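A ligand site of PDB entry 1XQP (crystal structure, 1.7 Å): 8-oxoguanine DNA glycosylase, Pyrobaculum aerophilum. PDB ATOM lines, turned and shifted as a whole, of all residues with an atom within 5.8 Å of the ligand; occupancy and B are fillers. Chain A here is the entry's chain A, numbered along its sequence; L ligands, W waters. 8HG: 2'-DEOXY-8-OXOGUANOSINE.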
ATOM      1  N   ASP A  29      12.492  -3.912  40.207  1.00  0.00           N
ATOM      2  CA  ASP A  29      12.407  -4.719  38.974  1.00  0.00           C
ATOM      3  C   ASP A  29      13.807  -4.782  38.328  1.00  0.00           C
ATOM      4  O   ASP A  29      14.410  -3.762  38.067  1.00  0.00           O
ATOM      5  CB  ASP A  29      11.401  -4.044  38.066  1.00  0.00           C
ATOM      6  CG  ASP A  29      11.199  -4.741  36.733  1.00  0.00           C
ATOM      7  OD1 ASP A  29      11.890  -5.705  36.328  1.00  0.00           O
ATOM      8  OD2 ASP A  29      10.281  -4.301  36.033  1.00  0.00           O
ATOM      9  N   GLN A  31      14.631  -5.216  35.387  1.00  0.00           N
ATOM     10  CA  GLN A  31      14.509  -4.411  34.166  1.00  0.00           C
ATOM     11  C   GLN A  31      14.738  -2.883  34.388  1.00  0.00           C
ATOM     12  O   GLN A  31      15.335  -2.198  33.533  1.00  0.00           O
ATOM     13  CB  GLN A  31      13.131  -4.656  33.491  1.00  0.00           C
ATOM     14  CG  GLN A  31      12.843  -6.170  33.227  1.00  0.00           C
ATOM     15  CD  GLN A  31      11.465  -6.458  32.632  1.00  0.00           C
ATOM     16  OE1 GLN A  31      11.349  -7.316  31.748  1.00  0.00           O
ATOM     17  NE2 GLN A  31      10.429  -5.827  33.147  1.00  0.00           N
ATOM     18  N   ALA A  55      12.338  -2.438  23.863  1.00  0.00           N
ATOM     19  CA  ALA A  55      10.958  -2.785  24.239  1.00  0.00           C
ATOM     20  C   ALA A  55      10.125  -3.187  22.994  1.00  0.00           C
ATOM     21  O   ALA A  55       9.391  -4.197  23.023  1.00  0.00           O
ATOM     22  CB  ALA A  55      10.308  -1.619  24.958  1.00  0.00           C
ATOM     23  N   SER A  58      10.794  -6.799  22.072  1.00  0.00           N
ATOM     24  CA  SER A  58      10.873  -7.728  23.205  1.00  0.00           C
ATOM     25  C   SER A  58       9.724  -8.738  23.093  1.00  0.00           C
ATOM     26  O   SER A  58       8.770  -8.677  23.870  1.00  0.00           O
ATOM     27  CB  SER A  58      10.834  -6.952  24.539  1.00  0.00           C
ATOM     28  OG  SER A  58      12.052  -6.251  24.818  1.00  0.00           O
ATOM     29  N   TYR A  59       9.827  -9.640  22.131  1.00  0.00           N
ATOM     30  CA  TYR A  59       8.808 -10.654  21.813  1.00  0.00           C
ATOM     31  C   TYR A  59       9.463 -11.925  21.245  1.00  0.00           C
ATOM     32  O   TYR A  59      10.562 -11.879  20.718  1.00  0.00           O
ATOM     33  CB  TYR A  59       7.752 -10.085  20.840  1.00  0.00           C
ATOM     34  CG  TYR A  59       8.274  -9.706  19.449  1.00  0.00           C
ATOM     35  CD1 TYR A  59       8.492 -10.669  18.472  1.00  0.00           C
ATOM     36  CD2 TYR A  59       8.501  -8.361  19.084  1.00  0.00           C
ATOM     37  CE1 TYR A  59       8.966 -10.351  17.182  1.00  0.00           C
ATOM     38  CE2 TYR A  59       8.986  -8.023  17.791  1.00  0.00           C
ATOM     39  CZ  TYR A  59       9.210  -9.014  16.853  1.00  0.00           C
ATOM     40  OH  TYR A  59       9.682  -8.698  15.577  1.00  0.00           O
ATOM     41  N   ARG A  60       8.774 -13.065  21.363  1.00  0.00           N
ATOM     42  CA  ARG A  60       9.329 -14.351  20.895  1.00  0.00           C
ATOM     43  C   ARG A  60      10.782 -14.565  21.322  1.00  0.00           C
ATOM     44  O   ARG A  60      11.677 -14.837  20.501  1.00  0.00           O
ATOM     45  CB  ARG A  60       9.175 -14.465  19.383  1.00  0.00           C
ATOM     46  CG  ARG A  60       7.747 -14.361  18.923  1.00  0.00           C
ATOM     47  CD  ARG A  60       7.600 -14.304  17.422  1.00  0.00           C
ATOM     48  NE  ARG A  60       8.043 -15.542  16.795  1.00  0.00           N
ATOM     49  CZ  ARG A  60       8.605 -15.633  15.582  1.00  0.00           C
ATOM     50  NH1 ARG A  60       8.813 -14.542  14.833  1.00  0.00           N
ATOM     51  NH2 ARG A  60       8.957 -16.833  15.114  1.00  0.00           N
ATOM     52  N   LEU A  61      11.002 -14.457  22.626  1.00  0.00           N
ATOM     53  CA  LEU A  61      12.316 -14.600  23.217  1.00  0.00           C
ATOM     54  C   LEU A  61      12.603 -16.066  23.459  1.00  0.00           C
ATOM     55  O   LEU A  61      11.691 -16.902  23.554  1.00  0.00           O
ATOM     56  CB  LEU A  61      12.408 -13.817  24.541  1.00  0.00           C
ATOM     57  CG  LEU A  61      11.989 -12.342  24.534  1.00  0.00           C
ATOM     58  CD1 LEU A  61      11.903 -11.780  25.969  1.00  0.00           C
ATOM     59  CD2 LEU A  61      12.943 -11.488  23.698  1.00  0.00           C
ATOM     60  N   GLY A  65      11.971 -12.738  29.926  1.00  0.00           N
ATOM     61  CA  GLY A  65      12.008 -11.267  29.806  1.00  0.00           C
ATOM     62  C   GLY A  65      13.140 -10.649  30.623  1.00  0.00           C
ATOM     63  O   GLY A  65      13.968  -9.915  30.064  1.00  0.00           O
ATOM     64  N   GLU A  66      13.225 -10.971  31.914  1.00  0.00           N
ATOM     65  CA  GLU A  66      14.253 -10.374  32.809  1.00  0.00           C
ATOM     66  C   GLU A  66      15.697 -10.626  32.365  1.00  0.00           C
ATOM     67  O   GLU A  66      16.551  -9.733  32.472  1.00  0.00           O
ATOM     68  CB  GLU A  66      14.071 -10.825  34.277  1.00  0.00           C
ATOM     69  CG  GLU A  66      12.745 -10.392  34.906  1.00  0.00           C
ATOM     70  CD  GLU A  66      11.660 -11.478  34.842  1.00  0.00           C
ATOM     71  OE1 GLU A  66      11.594 -12.212  33.845  1.00  0.00           O
ATOM     72  OE2 GLU A  66      10.853 -11.605  35.806  1.00  0.00           O
ATOM     73  N   HIS A  68      16.731 -11.208  29.236  1.00  0.00           N
ATOM     74  CA  HIS A  68      16.887 -10.450  27.980  1.00  0.00           C
ATOM     75  C   HIS A  68      17.275  -8.988  28.308  1.00  0.00           C
ATOM     76  O   HIS A  68      18.261  -8.466  27.754  1.00  0.00           O
ATOM     77  CB  HIS A  68      15.588 -10.591  27.165  1.00  0.00           C
ATOM     78  CG  HIS A  68      15.268  -9.446  26.261  1.00  0.00           C
ATOM     79  ND1 HIS A  68      16.037  -9.121  25.168  1.00  0.00           N
ATOM     80  CD2 HIS A  68      14.205  -8.616  26.238  1.00  0.00           C
ATOM     81  CE1 HIS A  68      15.483  -8.102  24.533  1.00  0.00           C
ATOM     82  NE2 HIS A  68      14.367  -7.774  25.153  1.00  0.00           N
ATOM     83  N   TRP A  69      16.570  -8.404  29.276  1.00  0.00           N
ATOM     84  CA  TRP A  69      16.839  -7.028  29.727  1.00  0.00           C
ATOM     85  C   TRP A  69      18.216  -6.888  30.417  1.00  0.00           C
ATOM     86  O   TRP A  69      18.939  -5.908  30.195  1.00  0.00           O
ATOM     87  CB  TRP A  69      15.687  -6.489  30.595  1.00  0.00           C
ATOM     88  CG  TRP A  69      14.509  -6.078  29.743  1.00  0.00           C
ATOM     89  CD1 TRP A  69      13.419  -6.863  29.382  1.00  0.00           C
ATOM     90  CD2 TRP A  69      14.397  -4.876  28.975  1.00  0.00           C
ATOM     91  NE1 TRP A  69      12.602  -6.176  28.522  1.00  0.00           N
ATOM     92  CE2 TRP A  69      13.161  -4.939  28.272  1.00  0.00           C
ATOM     93  CE3 TRP A  69      15.151  -3.690  28.908  1.00  0.00           C
ATOM     94  CZ2 TRP A  69      12.716  -3.905  27.451  1.00  0.00           C
ATOM     95  CZ3 TRP A  69      14.727  -2.685  28.065  1.00  0.00           C
ATOM     96  CH2 TRP A  69      13.516  -2.789  27.345  1.00  0.00           C
ATOM     97  N   LYS A 140       0.095  -5.011  23.083  1.00  0.00           N
ATOM     98  CA  LYS A 140       0.990  -5.244  24.240  1.00  0.00           C
ATOM     99  C   LYS A 140       2.366  -4.567  24.104  1.00  0.00           C
ATOM    100  O   LYS A 140       2.857  -4.009  25.060  1.00  0.00           O
ATOM    101  CB  LYS A 140       1.138  -6.750  24.582  1.00  0.00           C
ATOM    102  CG  LYS A 140       1.601  -7.702  23.479  1.00  0.00           C
ATOM    103  CD  LYS A 140       1.869  -9.086  24.055  1.00  0.00           C
ATOM    104  CE  LYS A 140       1.948 -10.184  22.997  1.00  0.00           C
ATOM    105  NZ  LYS A 140       2.666  -9.889  21.743  1.00  0.00           N
ATOM    106  N   THR A 141       2.960  -4.605  22.917  1.00  0.00           N
ATOM    107  CA  THR A 141       4.318  -4.103  22.805  1.00  0.00           C
ATOM    108  C   THR A 141       4.317  -2.579  22.895  1.00  0.00           C
ATOM    109  O   THR A 141       5.239  -2.030  23.460  1.00  0.00           O
ATOM    110  CB  THR A 141       5.068  -4.656  21.537  1.00  0.00           C
ATOM    111  OG1 THR A 141       5.497  -6.017  21.784  1.00  0.00           O
ATOM    112  CG2 THR A 141       6.329  -3.883  21.191  1.00  0.00           C
ATOM    113  N   PHE A 144       3.697  -1.636  26.798  1.00  0.00           N
ATOM    114  CA  PHE A 144       4.931  -2.012  27.512  1.00  0.00           C
ATOM    115  C   PHE A 144       6.102  -0.986  27.247  1.00  0.00           C
ATOM    116  O   PHE A 144       6.808  -0.570  28.168  1.00  0.00           O
ATOM    117  CB  PHE A 144       5.343  -3.445  27.185  1.00  0.00           C
ATOM    118  CG  PHE A 144       6.694  -3.796  27.709  1.00  0.00           C
ATOM    119  CD1 PHE A 144       6.921  -3.791  29.085  1.00  0.00           C
ATOM    120  CD2 PHE A 144       7.729  -4.180  26.854  1.00  0.00           C
ATOM    121  CE1 PHE A 144       8.194  -4.116  29.573  1.00  0.00           C
ATOM    122  CE2 PHE A 144       8.961  -4.534  27.355  1.00  0.00           C
ATOM    123  CZ  PHE A 144       9.215  -4.474  28.685  1.00  0.00           C
ATOM    124  N   LYS A 147       5.729   2.013  29.468  1.00  0.00           N
ATOM    125  CA  LYS A 147       6.236   1.664  30.810  1.00  0.00           C
ATOM    126  C   LYS A 147       7.779   1.761  30.867  1.00  0.00           C
ATOM    127  O   LYS A 147       8.348   2.422  31.761  1.00  0.00           O
ATOM    128  CB  LYS A 147       5.773   0.259  31.215  1.00  0.00           C
ATOM    129  CG  LYS A 147       6.455  -0.274  32.439  1.00  0.00           C
ATOM    130  CD  LYS A 147       5.734  -1.516  32.906  1.00  0.00           C
ATOM    131  CE  LYS A 147       6.656  -2.396  33.688  1.00  0.00           C
ATOM    132  NZ  LYS A 147       5.892  -3.351  34.570  1.00  0.00           N
ATOM    133  N   TYR A 151      10.376   4.271  33.099  1.00  0.00           N
ATOM    134  CA  TYR A 151      11.581   3.838  33.807  1.00  0.00           C
ATOM    135  C   TYR A 151      12.775   4.785  33.441  1.00  0.00           C
ATOM    136  O   TYR A 151      13.444   5.290  34.348  1.00  0.00           O
ATOM    137  CB  TYR A 151      11.891   2.378  33.464  1.00  0.00           C
ATOM    138  CG  TYR A 151      11.113   1.298  34.183  1.00  0.00           C
ATOM    139  CD1 TYR A 151       9.922   1.536  34.917  1.00  0.00           C
ATOM    140  CD2 TYR A 151      11.560  -0.004  34.095  1.00  0.00           C
ATOM    141  CE1 TYR A 151       9.242   0.485  35.567  1.00  0.00           C
ATOM    142  CE2 TYR A 151      10.920  -1.036  34.731  1.00  0.00           C
ATOM    143  CZ  TYR A 151       9.755  -0.811  35.467  1.00  0.00           C
ATOM    144  OH  TYR A 151       9.133  -1.893  36.076  1.00  0.00           O
ATOM    145  N   PRO A 170      -0.240  -4.509  29.488  1.00  0.00           N
ATOM    146  CA  PRO A 170       0.224  -5.324  28.355  1.00  0.00           C
ATOM    147  C   PRO A 170      -0.052  -6.816  28.592  1.00  0.00           C
ATOM    148  O   PRO A 170       0.574  -7.420  29.519  1.00  0.00           O
ATOM    149  CB  PRO A 170       1.741  -4.990  28.218  1.00  0.00           C
ATOM    150  CG  PRO A 170       2.077  -4.062  29.400  1.00  0.00           C
ATOM    151  CD  PRO A 170       0.888  -4.093  30.363  1.00  0.00           C
ATOM    152  N   VAL A 171      -0.956  -7.389  27.775  1.00  0.00           N
ATOM    153  CA  VAL A 171      -1.422  -8.773  27.916  1.00  0.00           C
ATOM    154  C   VAL A 171      -0.511  -9.747  27.143  1.00  0.00           C
ATOM    155  O   VAL A 171      -0.812 -10.200  26.025  1.00  0.00           O
ATOM    156  CB  VAL A 171      -2.911  -8.949  27.474  1.00  0.00           C
ATOM    157  CG1 VAL A 171      -3.403 -10.378  27.728  1.00  0.00           C
ATOM    158  CG2 VAL A 171      -3.849  -7.928  28.163  1.00  0.00           C
ATOM    159  N   ASP A 172       0.665  -9.973  27.719  1.00  0.00           N
ATOM    160  CA  ASP A 172       1.556 -11.036  27.276  1.00  0.00           C
ATOM    161  C   ASP A 172       1.167 -12.385  27.922  1.00  0.00           C
ATOM    162  O   ASP A 172       0.210 -12.480  28.727  1.00  0.00           O
ATOM    163  CB  ASP A 172       3.016 -10.686  27.602  1.00  0.00           C
ATOM    164  CG  ASP A 172       3.369 -11.031  29.040  1.00  0.00           C
ATOM    165  OD1 ASP A 172       2.661 -10.562  29.957  1.00  0.00           O
ATOM    166  OD2 ASP A 172       4.318 -11.797  29.324  1.00  0.00           O
ATOM    167  N   VAL A 175       1.118 -12.288  31.867  1.00  0.00           N
ATOM    168  CA  VAL A 175      -0.075 -11.590  32.392  1.00  0.00           C
ATOM    169  C   VAL A 175      -1.345 -12.442  32.208  1.00  0.00           C
ATOM    170  O   VAL A 175      -2.117 -12.583  33.167  1.00  0.00           O
ATOM    171  CB  VAL A 175      -0.211 -10.148  31.806  1.00  0.00           C
ATOM    172  CG1 VAL A 175      -1.624  -9.554  32.050  1.00  0.00           C
ATOM    173  CG2 VAL A 175       0.867  -9.222  32.379  1.00  0.00           C
ATOM    174  N   ASP A 218       0.892  -3.941  36.210  1.00  0.00           N
ATOM    175  CA  ASP A 218       1.750  -4.828  35.435  1.00  0.00           C
ATOM    176  C   ASP A 218       3.028  -5.215  36.188  1.00  0.00           C
ATOM    177  O   ASP A 218       3.474  -6.346  36.117  1.00  0.00           O
ATOM    178  CB  ASP A 218       2.162  -4.192  34.116  1.00  0.00           C
ATOM    179  CG  ASP A 218       3.015  -5.119  33.284  1.00  0.00           C
ATOM    180  OD1 ASP A 218       2.429  -6.148  32.804  1.00  0.00           O
ATOM    181  OD2 ASP A 218       4.265  -4.940  33.098  1.00  0.00           O
ATOM    182  N   TRP A 222       4.223  -9.058  37.153  1.00  0.00           N
ATOM    183  CA  TRP A 222       5.500  -9.562  36.688  1.00  0.00           C
ATOM    184  C   TRP A 222       6.390 -10.030  37.855  1.00  0.00           C
ATOM    185  O   TRP A 222       7.000 -11.101  37.799  1.00  0.00           O
ATOM    186  CB  TRP A 222       6.195  -8.599  35.668  1.00  0.00           C
ATOM    187  CG  TRP A 222       5.888  -9.051  34.218  1.00  0.00           C
ATOM    188  CD1 TRP A 222       4.647  -9.128  33.606  1.00  0.00           C
ATOM    189  CD2 TRP A 222       6.824  -9.613  33.269  1.00  0.00           C
ATOM    190  NE1 TRP A 222       4.780  -9.671  32.345  1.00  0.00           N
ATOM    191  CE2 TRP A 222       6.091  -9.948  32.104  1.00  0.00           C
ATOM    192  CE3 TRP A 222       8.221  -9.829  33.284  1.00  0.00           C
ATOM    193  CZ2 TRP A 222       6.707 -10.537  30.971  1.00  0.00           C
ATOM    194  CZ3 TRP A 222       8.821 -10.374  32.149  1.00  0.00           C
ATOM    195  CH2 TRP A 222       8.061 -10.731  31.013  1.00  0.00           C
HETATM  196  O6  8HG L   1       7.636  -6.234  32.609  1.00  0.00           O
HETATM  197  C6  8HG L   1       7.152  -6.690  31.582  1.00  0.00           C
HETATM  198  N1  8HG L   1       5.750  -6.685  31.479  1.00  0.00           N
HETATM  199  C2  8HG L   1       5.050  -7.147  30.322  1.00  0.00           C
HETATM  200  N2  8HG L   1       3.670  -7.118  30.376  1.00  0.00           N
HETATM  201  N3  8HG L   1       5.714  -7.614  29.285  1.00  0.00           N
HETATM  202  C4  8HG L   1       7.074  -7.639  29.351  1.00  0.00           C
HETATM  203  C5  8HG L   1       7.811  -7.239  30.425  1.00  0.00           C
HETATM  204  N7  8HG L   1       9.203  -7.428  30.142  1.00  0.00           N
HETATM  205  C8  8HG L   1       9.283  -7.945  28.813  1.00  0.00           C
HETATM  206  O20 8HG L   1      10.310  -8.200  28.177  1.00  0.00           O
HETATM  207  N9  8HG L   1       7.955  -8.116  28.349  1.00  0.00           N
HETATM  208  C1' 8HG L   1       7.580  -8.600  27.022  1.00  0.00           C
HETATM  209  O4' 8HG L   1       7.090  -7.451  26.356  1.00  0.00           O
HETATM  210  C2' 8HG L   1       6.492  -9.637  26.908  1.00  0.00           C
HETATM  211  C3' 8HG L   1       5.868  -9.333  25.544  1.00  0.00           C
HETATM  212  O3' 8HG L   1       6.516  -9.962  24.454  1.00  0.00           O
HETATM  213  C4' 8HG L   1       6.022  -7.794  25.427  1.00  0.00           C
HETATM  214  C5' 8HG L   1       4.655  -7.107  25.697  1.00  0.00           C
HETATM  215  O5' 8HG L   1       3.998  -7.472  26.834  1.00  0.00           O
HETATM  216  O   HOH W   1       7.828  -5.559  35.407  1.00  0.00           O
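The side-chain hydroxyl of Ser 58 is in hydrogen-bond range of a ring nitrogen (NE2) of His 68, at 2.8 Å.
The backbone NH (N) of Gln 31 is in hydrogen-bond range of the side-chain carboxylate (OD1) of Asp 29 (2.9 Å).
The side-chain carboxylate (OD2) of Asp 218 lies within salt-bridge range of the side-chain amino group (NZ) of Lys 147, 2.7 Å away.
The indole nitrogen of Trp 222 lies within hydrogen-bond range of the side-chain carboxylate of Asp 172 (3.3 Å).
The side-chain carboxylate of Asp 172 lies within hydrogen-bond range of the backbone NH of Val 175, 3.0 Å away.
The indole nitrogen (NE1) of Trp 222 lies close to a nitrogen (N1) of the ligand.
CA of Tyr 59 touches O3' of the ligand (3.6 Å).
Gly 65 touches the ligand.
O of Lys 140 touches C5' of the ligand, at 3.6 Å.
Phe 144 touches the ligand (CE1 to C5, 3.3 Å).
NZ of Lys 147 touches O6 of the ligand, at 3.9 Å.
Asp 172 touches the ligand.
Hydrophobic or aromatic side chains within 4 Å of the ligand: Tyr 59, Trp 69, Phe 144, Pro 170 and Trp 222.
Of the 22 residues printed, 12 come within 4 Å of the ligand.
The nearest printed residue that does not touch the ligand is Val 175 (4.04 Å).
An oxygen (O3') of the ligand is in hydrogen-bond range of the backbone carbonyl oxygen of Ser 58, at 2.7 Å.
The side-chain amide oxygen of Gln 31 sits at hydrogen-bond distance from a nitrogen (N7) of the ligand (2.7 Å).
OD2 of Asp 218 sits at hydrogen-bond distance from N1 of the ligand, at 2.8 Å.
The indole nitrogen (NE1) of Trp 69 is in hydrogen-bond range of an oxygen (O20) of the ligand (3.1 Å).
N2 of the ligand sits at hydrogen-bond distance from O of Pro 170.
Water W1 lies within hydrogen-bond range of the side-chain carboxylate of Asp 29 (2.8 Å), an oxygen (O6) of the ligand (2.9 Å), the side-chain amino group of Lys 147 (3.1 Å) and the side-chain amide nitrogen of Gln 31 (3.5 Å).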
